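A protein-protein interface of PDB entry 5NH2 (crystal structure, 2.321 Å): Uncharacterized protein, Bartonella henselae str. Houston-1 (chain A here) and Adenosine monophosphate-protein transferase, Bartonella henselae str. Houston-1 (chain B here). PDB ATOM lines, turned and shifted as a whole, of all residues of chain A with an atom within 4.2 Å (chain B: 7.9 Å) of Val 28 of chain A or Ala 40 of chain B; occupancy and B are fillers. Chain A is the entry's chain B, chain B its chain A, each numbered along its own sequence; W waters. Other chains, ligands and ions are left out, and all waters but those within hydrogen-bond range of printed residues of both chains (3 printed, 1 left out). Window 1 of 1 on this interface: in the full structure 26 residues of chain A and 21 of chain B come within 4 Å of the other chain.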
ATOM      1  N   ALA A  24      36.461  -0.304   7.986  1.00  0.00           N
ATOM      2  CA  ALA A  24      35.246  -1.080   7.772  1.00  0.00           C
ATOM      3  C   ALA A  24      33.990  -0.272   8.094  1.00  0.00           C
ATOM      4  O   ALA A  24      33.012  -0.308   7.334  1.00  0.00           O
ATOM      5  CB  ALA A  24      35.297  -2.338   8.600  1.00  0.00           C
ATOM      6  N   VAL A  25      34.015   0.488   9.196  1.00  0.00           N
ATOM      7  CA  VAL A  25      32.898   1.371   9.555  1.00  0.00           C
ATOM      8  C   VAL A  25      32.810   2.568   8.592  1.00  0.00           C
ATOM      9  O   VAL A  25      31.716   3.006   8.208  1.00  0.00           O
ATOM     10  CB  VAL A  25      33.052   1.802  11.036  1.00  0.00           C
ATOM     11  CG1 VAL A  25      32.182   3.012  11.371  1.00  0.00           C
ATOM     12  CG2 VAL A  25      32.733   0.609  11.984  1.00  0.00           C
ATOM     13  N   ASP A  26      33.954   3.114   8.178  1.00  0.00           N
ATOM     14  CA  ASP A  26      33.914   4.194   7.201  1.00  0.00           C
ATOM     15  C   ASP A  26      33.291   3.726   5.898  1.00  0.00           C
ATOM     16  O   ASP A  26      32.540   4.473   5.266  1.00  0.00           O
ATOM     17  CB  ASP A  26      35.316   4.739   6.931  1.00  0.00           C
ATOM     18  CG  ASP A  26      35.837   5.635   8.071  1.00  0.00           C
ATOM     19  OD1 ASP A  26      35.068   5.944   9.008  1.00  0.00           O
ATOM     20  OD2 ASP A  26      37.019   6.031   8.028  1.00  0.00           O
ATOM     21  N   ALA A  27      33.614   2.499   5.470  1.00  0.00           N
ATOM     22  CA  ALA A  27      33.041   1.946   4.249  1.00  0.00           C
ATOM     23  C   ALA A  27      31.547   1.713   4.403  1.00  0.00           C
ATOM     24  O   ALA A  27      30.787   1.970   3.468  1.00  0.00           O
ATOM     25  CB  ALA A  27      33.740   0.641   3.856  1.00  0.00           C
ATOM     26  N   VAL A  28      31.101   1.256   5.576  1.00  0.00           N
ATOM     27  CA  VAL A  28      29.662   1.072   5.780  1.00  0.00           C
ATOM     28  C   VAL A  28      28.929   2.399   5.672  1.00  0.00           C
ATOM     29  O   VAL A  28      27.861   2.501   5.046  1.00  0.00           O
ATOM     30  CB  VAL A  28      29.383   0.411   7.134  1.00  0.00           C
ATOM     31  CG1 VAL A  28      27.869   0.628   7.557  1.00  0.00           C
ATOM     32  CG2 VAL A  28      29.770  -1.048   7.050  1.00  0.00           C
ATOM     33  N   ILE A  29      29.465   3.425   6.324  1.00  0.00           N
ATOM     34  CA  ILE A  29      28.818   4.733   6.290  1.00  0.00           C
ATOM     35  C   ILE A  29      28.835   5.284   4.863  1.00  0.00           C
ATOM     36  O   ILE A  29      27.818   5.768   4.337  1.00  0.00           O
ATOM     37  CB  ILE A  29      29.514   5.670   7.301  1.00  0.00           C
ATOM     38  CG1 ILE A  29      29.242   5.187   8.750  1.00  0.00           C
ATOM     39  CG2 ILE A  29      29.087   7.130   7.132  1.00  0.00           C
ATOM     40  CD1 ILE A  29      29.837   6.096   9.873  1.00  0.00           C
ATOM     41  N   SER A  30      29.992   5.173   4.202  1.00  0.00           N
ATOM     42  CA  SER A  30      30.164   5.757   2.883  1.00  0.00           C
ATOM     43  C   SER A  30      29.239   5.111   1.872  1.00  0.00           C
ATOM     44  O   SER A  30      28.655   5.813   1.050  1.00  0.00           O
ATOM     45  CB  SER A  30      31.610   5.610   2.405  1.00  0.00           C
ATOM     46  OG  SER A  30      31.687   5.814   0.987  1.00  0.00           O
ATOM     47  N   THR A  31      29.097   3.771   1.914  1.00  0.00           N
ATOM     48  CA  THR A  31      28.378   3.078   0.842  1.00  0.00           C
ATOM     49  C   THR A  31      26.889   3.408   0.864  1.00  0.00           C
ATOM     50  O   THR A  31      26.238   3.403  -0.193  1.00  0.00           O
ATOM     51  CB  THR A  31      28.595   1.568   0.929  1.00  0.00           C
ATOM     52  OG1 THR A  31      28.243   0.970  -0.333  1.00  0.00           O
ATOM     53  CG2 THR A  31      27.762   0.913   2.101  1.00  0.00           C
ATOM     54  N   HIS A  32      26.356   3.722   2.053  1.00  0.00           N
ATOM     55  CA  HIS A  32      25.017   4.296   2.172  1.00  0.00           C
ATOM     56  C   HIS A  32      24.990   5.749   1.729  1.00  0.00           C
ATOM     57  O   HIS A  32      24.148   6.118   0.906  1.00  0.00           O
ATOM     58  CB  HIS A  32      24.497   4.146   3.614  1.00  0.00           C
ATOM     59  CG  HIS A  32      24.136   2.729   3.944  1.00  0.00           C
ATOM     60  ND1 HIS A  32      25.053   1.823   4.438  1.00  0.00           N
ATOM     61  CD2 HIS A  32      22.990   2.033   3.737  1.00  0.00           C
ATOM     62  CE1 HIS A  32      24.473   0.642   4.560  1.00  0.00           C
ATOM     63  NE2 HIS A  32      23.220   0.748   4.147  1.00  0.00           N
ATOM     64  N   LEU A  39      22.457   7.015   8.211  1.00  0.00           N
ATOM     65  CA  LEU A  39      22.100   5.925   9.110  1.00  0.00           C
ATOM     66  C   LEU A  39      21.441   6.475  10.369  1.00  0.00           C
ATOM     67  O   LEU A  39      21.701   7.608  10.794  1.00  0.00           O
ATOM     68  CB  LEU A  39      23.342   5.100   9.459  1.00  0.00           C
ATOM     69  CG  LEU A  39      24.079   4.503   8.237  1.00  0.00           C
ATOM     70  CD1 LEU A  39      25.305   3.683   8.687  1.00  0.00           C
ATOM     71  CD2 LEU A  39      23.098   3.634   7.446  1.00  0.00           C
ATOM     72  N   THR A  43      22.517   3.280  15.094  1.00  0.00           N
ATOM     73  CA  THR A  43      23.404   2.542  14.206  1.00  0.00           C
ATOM     74  C   THR A  43      24.801   3.140  14.234  1.00  0.00           C
ATOM     75  O   THR A  43      25.813   2.432  14.411  1.00  0.00           O
ATOM     76  CB  THR A  43      22.799   2.562  12.799  1.00  0.00           C
ATOM     77  OG1 THR A  43      21.441   2.096  12.888  1.00  0.00           O
ATOM     78  CG2 THR A  43      23.574   1.663  11.832  1.00  0.00           C
ATOM     79  N   LEU A  47      28.188   1.148  15.685  1.00  0.00           N
ATOM     80  CA  LEU A  47      29.347   1.074  14.786  1.00  0.00           C
ATOM     81  C   LEU A  47      30.552   1.795  15.391  1.00  0.00           C
ATOM     82  O   LEU A  47      31.686   1.291  15.358  1.00  0.00           O
ATOM     83  CB  LEU A  47      29.004   1.692  13.419  1.00  0.00           C
ATOM     84  CG  LEU A  47      27.929   1.045  12.531  1.00  0.00           C
ATOM     85  CD1 LEU A  47      27.581   1.905  11.323  1.00  0.00           C
ATOM     86  CD2 LEU A  47      28.444  -0.304  12.056  1.00  0.00           C
ATOM     87  N   GLU B  33      15.284   2.913   7.634  1.00  0.00           N
ATOM     88  CA  GLU B  33      16.174   2.938   8.793  1.00  0.00           C
ATOM     89  C   GLU B  33      16.503   1.531   9.286  1.00  0.00           C
ATOM     90  O   GLU B  33      17.666   1.247   9.626  1.00  0.00           O
ATOM     91  CB  GLU B  33      15.541   3.772   9.908  1.00  0.00           C
ATOM     92  CG  GLU B  33      15.533   5.269   9.650  1.00  0.00           C
ATOM     93  CD  GLU B  33      14.795   6.053  10.729  1.00  0.00           C
ATOM     94  OE1 GLU B  33      14.055   5.457  11.537  1.00  0.00           O
ATOM     95  OE2 GLU B  33      14.971   7.275  10.787  1.00  0.00           O
ATOM     96  N   LYS B  34      15.507   0.626   9.295  1.00  0.00           N
ATOM     97  CA  LYS B  34      15.750  -0.730   9.783  1.00  0.00           C
ATOM     98  C   LYS B  34      16.521  -1.585   8.769  1.00  0.00           C
ATOM     99  O   LYS B  34      17.453  -2.316   9.149  1.00  0.00           O
ATOM    100  CB  LYS B  34      14.424  -1.399  10.175  1.00  0.00           C
ATOM    101  CG  LYS B  34      14.568  -2.861  10.674  1.00  0.00           C
ATOM    102  CD  LYS B  34      15.214  -2.928  12.081  1.00  0.00           C
ATOM    103  CE  LYS B  34      15.956  -4.257  12.246  1.00  0.00           C
ATOM    104  NZ  LYS B  34      16.400  -4.581  13.623  1.00  0.00           N
ATOM    105  N   CYS B  35      16.127  -1.549   7.479  1.00  0.00           N
ATOM    106  CA  CYS B  35      16.955  -2.172   6.441  1.00  0.00           C
ATOM    107  C   CYS B  35      18.392  -1.612   6.459  1.00  0.00           C
ATOM    108  O   CYS B  35      19.361  -2.366   6.352  1.00  0.00           O
ATOM    109  CB  CYS B  35      16.317  -1.985   5.054  1.00  0.00           C
ATOM    110  SG  CYS B  35      17.425  -2.520   3.629  1.00  0.00           S
ATOM    111  N   SER B  36      18.552  -0.305   6.632  1.00  0.00           N
ATOM    112  CA  SER B  36      19.906   0.247   6.681  1.00  0.00           C
ATOM    113  C   SER B  36      20.690  -0.311   7.852  1.00  0.00           C
ATOM    114  O   SER B  36      21.892  -0.576   7.732  1.00  0.00           O
ATOM    115  CB  SER B  36      19.861   1.766   6.795  1.00  0.00           C
ATOM    116  OG  SER B  36      19.908   2.272   5.498  1.00  0.00           O
ATOM    117  N   HIS B  37      20.012  -0.464   8.991  1.00  0.00           N
ATOM    118  CA  HIS B  37      20.650  -0.893  10.229  1.00  0.00           C
ATOM    119  C   HIS B  37      21.128  -2.331  10.119  1.00  0.00           C
ATOM    120  O   HIS B  37      22.296  -2.644  10.450  1.00  0.00           O
ATOM    121  CB  HIS B  37      19.650  -0.724  11.369  1.00  0.00           C
ATOM    122  CG  HIS B  37      20.104  -1.283  12.679  1.00  0.00           C
ATOM    123  ND1 HIS B  37      20.550  -0.482  13.706  1.00  0.00           N
ATOM    124  CD2 HIS B  37      20.113  -2.548  13.153  1.00  0.00           C
ATOM    125  CE1 HIS B  37      20.835  -1.235  14.752  1.00  0.00           C
ATOM    126  NE2 HIS B  37      20.577  -2.492  14.442  1.00  0.00           N
ATOM    127  N   ASP B  38      20.253  -3.207   9.582  1.00  0.00           N
ATOM    128  CA  ASP B  38      20.608  -4.614   9.421  1.00  0.00           C
ATOM    129  C   ASP B  38      21.700  -4.779   8.382  1.00  0.00           C
ATOM    130  O   ASP B  38      22.592  -5.615   8.555  1.00  0.00           O
ATOM    131  CB  ASP B  38      19.369  -5.435   9.039  1.00  0.00           C
ATOM    132  CG  ASP B  38      18.405  -5.646  10.233  1.00  0.00           C
ATOM    133  OD1 ASP B  38      18.852  -5.470  11.392  1.00  0.00           O
ATOM    134  OD2 ASP B  38      17.200  -5.980  10.015  1.00  0.00           O
ATOM    135  N   THR B  39      21.639  -3.998   7.279  1.00  0.00           N
ATOM    136  CA  THR B  39      22.674  -4.087   6.244  1.00  0.00           C
ATOM    137  C   THR B  39      24.022  -3.618   6.770  1.00  0.00           C
ATOM    138  O   THR B  39      25.064  -4.162   6.381  1.00  0.00           O
ATOM    139  CB  THR B  39      22.280  -3.267   5.028  1.00  0.00           C
ATOM    140  OG1 THR B  39      21.047  -3.767   4.532  1.00  0.00           O
ATOM    141  CG2 THR B  39      23.318  -3.375   3.940  1.00  0.00           C
ATOM    142  N   ALA B  40      24.030  -2.634   7.680  1.00  0.00           N
ATOM    143  CA  ALA B  40      25.287  -2.311   8.367  1.00  0.00           C
ATOM    144  C   ALA B  40      25.814  -3.519   9.142  1.00  0.00           C
ATOM    145  O   ALA B  40      27.007  -3.880   9.053  1.00  0.00           O
ATOM    146  CB  ALA B  40      25.088  -1.123   9.307  1.00  0.00           C
ATOM    147  N   LYS B  41      24.935  -4.176   9.888  1.00  0.00           N
ATOM    148  CA  LYS B  41      25.398  -5.341  10.636  1.00  0.00           C
ATOM    149  C   LYS B  41      25.996  -6.380   9.691  1.00  0.00           C
ATOM    150  O   LYS B  41      27.105  -6.882   9.943  1.00  0.00           O
ATOM    151  CB  LYS B  41      24.254  -5.944  11.470  1.00  0.00           C
ATOM    152  CG  LYS B  41      24.708  -7.179  12.272  1.00  0.00           C
ATOM    153  CD  LYS B  41      23.539  -8.059  12.705  1.00  0.00           C
ATOM    154  CE  LYS B  41      24.002  -9.360  13.355  1.00  0.00           C
ATOM    155  NZ  LYS B  41      22.881 -10.248  13.731  1.00  0.00           N
ATOM    156  N   ALA B  42      25.298  -6.662   8.561  1.00  0.00           N
ATOM    157  CA  ALA B  42      25.761  -7.674   7.604  1.00  0.00           C
ATOM    158  C   ALA B  42      27.094  -7.294   6.967  1.00  0.00           C
ATOM    159  O   ALA B  42      27.943  -8.156   6.768  1.00  0.00           O
ATOM    160  CB  ALA B  42      24.710  -7.955   6.502  1.00  0.00           C
ATOM    161  N   MET B  43      27.308  -6.026   6.607  1.00  0.00           N
ATOM    162  CA  MET B  43      28.627  -5.708   6.040  1.00  0.00           C
ATOM    163  C   MET B  43      29.750  -5.939   7.052  1.00  0.00           C
ATOM    164  O   MET B  43      30.828  -6.452   6.706  1.00  0.00           O
ATOM    165  CB  MET B  43      28.672  -4.269   5.542  1.00  0.00           C
ATOM    166  CG  MET B  43      27.665  -4.030   4.507  1.00  0.00           C
ATOM    167  SD  MET B  43      27.680  -2.321   4.031  1.00  0.00           S
ATOM    168  CE  MET B  43      29.341  -2.199   3.327  1.00  0.00           C
ATOM    169  N   ILE B  44      29.532  -5.555   8.312  1.00  0.00           N
ATOM    170  CA  ILE B  44      30.634  -5.776   9.243  1.00  0.00           C
ATOM    171  C   ILE B  44      30.948  -7.261   9.330  1.00  0.00           C
ATOM    172  O   ILE B  44      32.115  -7.660   9.267  1.00  0.00           O
ATOM    173  CB  ILE B  44      30.359  -5.150  10.616  1.00  0.00           C
ATOM    174  CG1 ILE B  44      30.927  -3.740  10.635  1.00  0.00           C
ATOM    175  CG2 ILE B  44      31.178  -5.871  11.689  1.00  0.00           C
ATOM    176  CD1 ILE B  44      30.069  -2.724  10.103  1.00  0.00           C
ATOM    177  N   ASN B  45      29.912  -8.112   9.351  1.00  0.00           N
ATOM    178  CA  ASN B  45      30.194  -9.535   9.492  1.00  0.00           C
ATOM    179  C   ASN B  45      30.777 -10.116   8.197  1.00  0.00           C
ATOM    180  O   ASN B  45      31.718 -10.904   8.233  1.00  0.00           O
ATOM    181  CB  ASN B  45      28.917 -10.247   9.948  1.00  0.00           C
ATOM    182  CG  ASN B  45      28.686 -10.114  11.460  1.00  0.00           C
ATOM    183  OD1 ASN B  45      29.209 -10.912  12.291  1.00  0.00           O
ATOM    184  ND2 ASN B  45      27.910  -9.104  11.830  1.00  0.00           N
ATOM    185  N   LEU B  46      30.252  -9.703   7.048  1.00  0.00           N
ATOM    186  CA  LEU B  46      30.786 -10.088   5.747  1.00  0.00           C
ATOM    187  C   LEU B  46      32.275  -9.839   5.656  1.00  0.00           C
ATOM    188  O   LEU B  46      32.998 -10.594   4.999  1.00  0.00           O
ATOM    189  CB  LEU B  46      30.077  -9.295   4.651  1.00  0.00           C
ATOM    190  CG  LEU B  46      30.117  -9.827   3.227  1.00  0.00           C
ATOM    191  CD1 LEU B  46      30.020 -11.393   3.105  1.00  0.00           C
ATOM    192  CD2 LEU B  46      28.954  -9.147   2.503  1.00  0.00           C
ATOM    193  N   ARG B  47      32.757  -8.775   6.304  1.00  0.00           N
ATOM    194  CA  ARG B  47      34.195  -8.522   6.270  1.00  0.00           C
ATOM    195  C   ARG B  47      35.006  -9.668   6.869  1.00  0.00           C
ATOM    196  O   ARG B  47      36.221  -9.696   6.682  1.00  0.00           O
ATOM    197  CB  ARG B  47      34.513  -7.199   6.978  1.00  0.00           C
ATOM    198  CG  ARG B  47      34.282  -5.978   6.099  1.00  0.00           C
ATOM    199  CD  ARG B  47      35.598  -5.217   5.887  1.00  0.00           C
ATOM    200  NE  ARG B  47      35.539  -4.110   4.922  1.00  0.00           N
ATOM    201  CZ  ARG B  47      36.517  -3.212   4.773  1.00  0.00           C
ATOM    202  NH1 ARG B  47      37.615  -3.275   5.534  1.00  0.00           N
ATOM    203  NH2 ARG B  47      36.397  -2.242   3.877  1.00  0.00           N
ATOM    204  N   LEU B  67      23.942  -9.344   2.488  1.00  0.00           N
ATOM    205  CA  LEU B  67      23.586  -7.979   2.905  1.00  0.00           C
ATOM    206  C   LEU B  67      22.114  -7.884   3.293  1.00  0.00           C
ATOM    207  O   LEU B  67      21.772  -7.188   4.254  1.00  0.00           O
ATOM    208  CB  LEU B  67      23.925  -6.923   1.817  1.00  0.00           C
ATOM    209  CG  LEU B  67      25.399  -6.759   1.384  1.00  0.00           C
ATOM    210  CD1 LEU B  67      25.595  -5.703   0.294  1.00  0.00           C
ATOM    211  CD2 LEU B  67      26.374  -6.528   2.566  1.00  0.00           C
ATOM    212  N   PHE B  68      21.229  -8.493   2.500  1.00  0.00           N
ATOM    213  CA  PHE B  68      19.795  -8.239   2.594  1.00  0.00           C
ATOM    214  C   PHE B  68      18.942  -9.401   3.114  1.00  0.00           C
ATOM    215  O   PHE B  68      17.708  -9.277   3.113  1.00  0.00           O
ATOM    216  CB  PHE B  68      19.298  -7.745   1.232  1.00  0.00           C
ATOM    217  CG  PHE B  68      19.970  -6.473   0.808  1.00  0.00           C
ATOM    218  CD1 PHE B  68      19.661  -5.271   1.441  1.00  0.00           C
ATOM    219  CD2 PHE B  68      20.952  -6.481  -0.193  1.00  0.00           C
ATOM    220  CE1 PHE B  68      20.326  -4.077   1.086  1.00  0.00           C
ATOM    221  CE2 PHE B  68      21.626  -5.298  -0.581  1.00  0.00           C
ATOM    222  CZ  PHE B  68      21.311  -4.084   0.065  1.00  0.00           C
ATOM    223  N   ARG B 159      25.538  -1.137  -3.640  1.00  0.00           N
ATOM    224  CA  ARG B 159      26.239  -1.618  -2.444  1.00  0.00           C
ATOM    225  C   ARG B 159      26.887  -2.976  -2.690  1.00  0.00           C
ATOM    226  O   ARG B 159      28.054  -3.199  -2.310  1.00  0.00           O
ATOM    227  CB  ARG B 159      25.275  -1.668  -1.260  1.00  0.00           C
ATOM    228  CG  ARG B 159      25.062  -0.297  -0.647  1.00  0.00           C
ATOM    229  CD  ARG B 159      23.966  -0.284   0.438  1.00  0.00           C
ATOM    230  NE  ARG B 159      22.650  -0.145  -0.148  1.00  0.00           N
ATOM    231  CZ  ARG B 159      21.504  -0.243   0.513  1.00  0.00           C
ATOM    232  NH1 ARG B 159      21.463  -0.508   1.835  1.00  0.00           N
ATOM    233  NH2 ARG B 159      20.390  -0.079  -0.169  1.00  0.00           N
ATOM    234  N   LEU B 163      31.101  -3.678  -2.960  1.00  0.00           N
ATOM    235  CA  LEU B 163      31.765  -4.714  -2.174  1.00  0.00           C
ATOM    236  C   LEU B 163      32.429  -5.767  -3.076  1.00  0.00           C
ATOM    237  O   LEU B 163      33.518  -6.272  -2.761  1.00  0.00           O
ATOM    238  CB  LEU B 163      30.775  -5.368  -1.213  1.00  0.00           C
ATOM    239  CG  LEU B 163      31.278  -5.480   0.235  1.00  0.00           C
ATOM    240  CD1 LEU B 163      30.191  -6.060   1.125  1.00  0.00           C
ATOM    241  CD2 LEU B 163      32.598  -6.278   0.365  1.00  0.00           C
ATOM    242  N   GLU B 166      35.711  -4.216  -4.297  1.00  0.00           N
ATOM    243  CA  GLU B 166      36.695  -4.084  -3.216  1.00  0.00           C
ATOM    244  C   GLU B 166      37.361  -5.421  -2.934  1.00  0.00           C
ATOM    245  O   GLU B 166      38.592  -5.510  -2.811  1.00  0.00           O
ATOM    246  CB  GLU B 166      36.039  -3.547  -1.927  1.00  0.00           C
ATOM    247  CG  GLU B 166      35.538  -2.095  -1.954  1.00  0.00           C
ATOM    248  CD  GLU B 166      34.540  -1.768  -0.814  1.00  0.00           C
ATOM    249  OE1 GLU B 166      34.337  -2.597   0.101  1.00  0.00           O
ATOM    250  OE2 GLU B 166      33.947  -0.671  -0.827  1.00  0.00           O
ATOM    251  N   SER B 179      35.180   4.644  -0.129  1.00  0.00           N
ATOM    252  CA  SER B 179      34.772   5.619   0.858  1.00  0.00           C
ATOM    253  C   SER B 179      35.409   6.977   0.609  1.00  0.00           C
ATOM    254  O   SER B 179      35.048   7.951   1.278  1.00  0.00           O
ATOM    255  CB  SER B 179      35.081   5.077   2.265  1.00  0.00           C
ATOM    256  OG  SER B 179      36.398   5.396   2.634  1.00  0.00           O
HETATM  257  O   HOH W   1      29.225  -1.640  -0.313  1.00  0.00           O
HETATM  258  O   HOH W   2      32.360   3.152   0.157  1.00  0.00           O
HETATM  259  O   HOH W   3      20.382   2.900  10.314  1.00  0.00           O
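Printed residues of chain A that touch a printed residue of chain B: Ala 24, Asp 26, Ala 27, Val 28, Ser 30, Thr 31, His 32, Leu 39, Thr 43 and Leu 47. Along chain A the printed residues that touch a printed residue of chain B span positions 24 to 47. Among the printed residues, 14 pairs touch across the chains. Among the printed residues, no Asp or Glu carboxylate lies within 4 Å of a Lys or Arg side-chain nitrogen of the other chain.
ND1 of His 37 of chain B sits at hydrogen-bond distance from OG1 of Thr 43 of chain A. A ring nitrogen (NE2) of His 32 of chain A lies within hydrogen-bond range of the guanidinium group (NH1) of Arg 159 of chain B (3.2 Å).
Printed residues of chain B within 4 Å of Ala 27 of chain A: Arg 47. Of the printed residues of chain B, Thr 31 of chain A touches Met 43 (3.7 Å) and Arg 159 (3.4 Å). Of chain A, only Val 28 comes within 4 Å of Ala 40 of chain B. Of the printed residues of chain A, Met 43 of chain B touches Val 28 and Thr 31. Leu 163 of chain B touches none of the printed residues of chain A. The nearest residue of chain B that does not touch Val 28 of chain A is Thr 39 of chain B (5.7 Å).
Water W1 bridges OG1 of Thr 31 of chain A (2.8 Å) and O of Arg 159 of chain B (2.8 Å). Water W2 bridges OG of Ser 30 of chain A and N of Ser 179 of chain B. Water W3 bridges the side-chain hydroxyl of Thr 43 of chain A (2.9 Å) and the backbone carbonyl oxygen of Glu 33 of chain B (3.3 Å).
Arg 47 of chain B touches Ala 24 of chain A (CZ to CA, 3.9 Å). CB of Ala 27 of chain A touches NH2 of Arg 47 of chain B, 3.9 Å away. CB of Ala 40 of chain B touches CG1 of Val 28 of chain A, at 3.7 Å. CG2 of Val 28 of chain A touches CB of Met 43 of chain B, at 3.7 Å. Ile 44 of chain B touches Val 28 of chain A (CD1 to CG2, 3.5 Å). Ser 30 of chain A touches Ser 179 of chain B. Thr 31 of chain A touches Met 43 of chain B (CG2 to CE, 3.7 Å). CG of Arg 159 of chain B touches OG1 of Thr 31 of chain A, at 3.4 Å. CB of Ser 36 of chain B touches CD2 of Leu 39 of chain A (3.8 Å). Leu 47 of chain A touches Ile 44 of chain B (CD2 to CD1, 3.5 Å).
The backbone carbonyl oxygen (O) of Val 28 of chain A lies within hydrogen-bond range of a ring nitrogen (ND1) of His 32 of chain A (3.0 Å).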
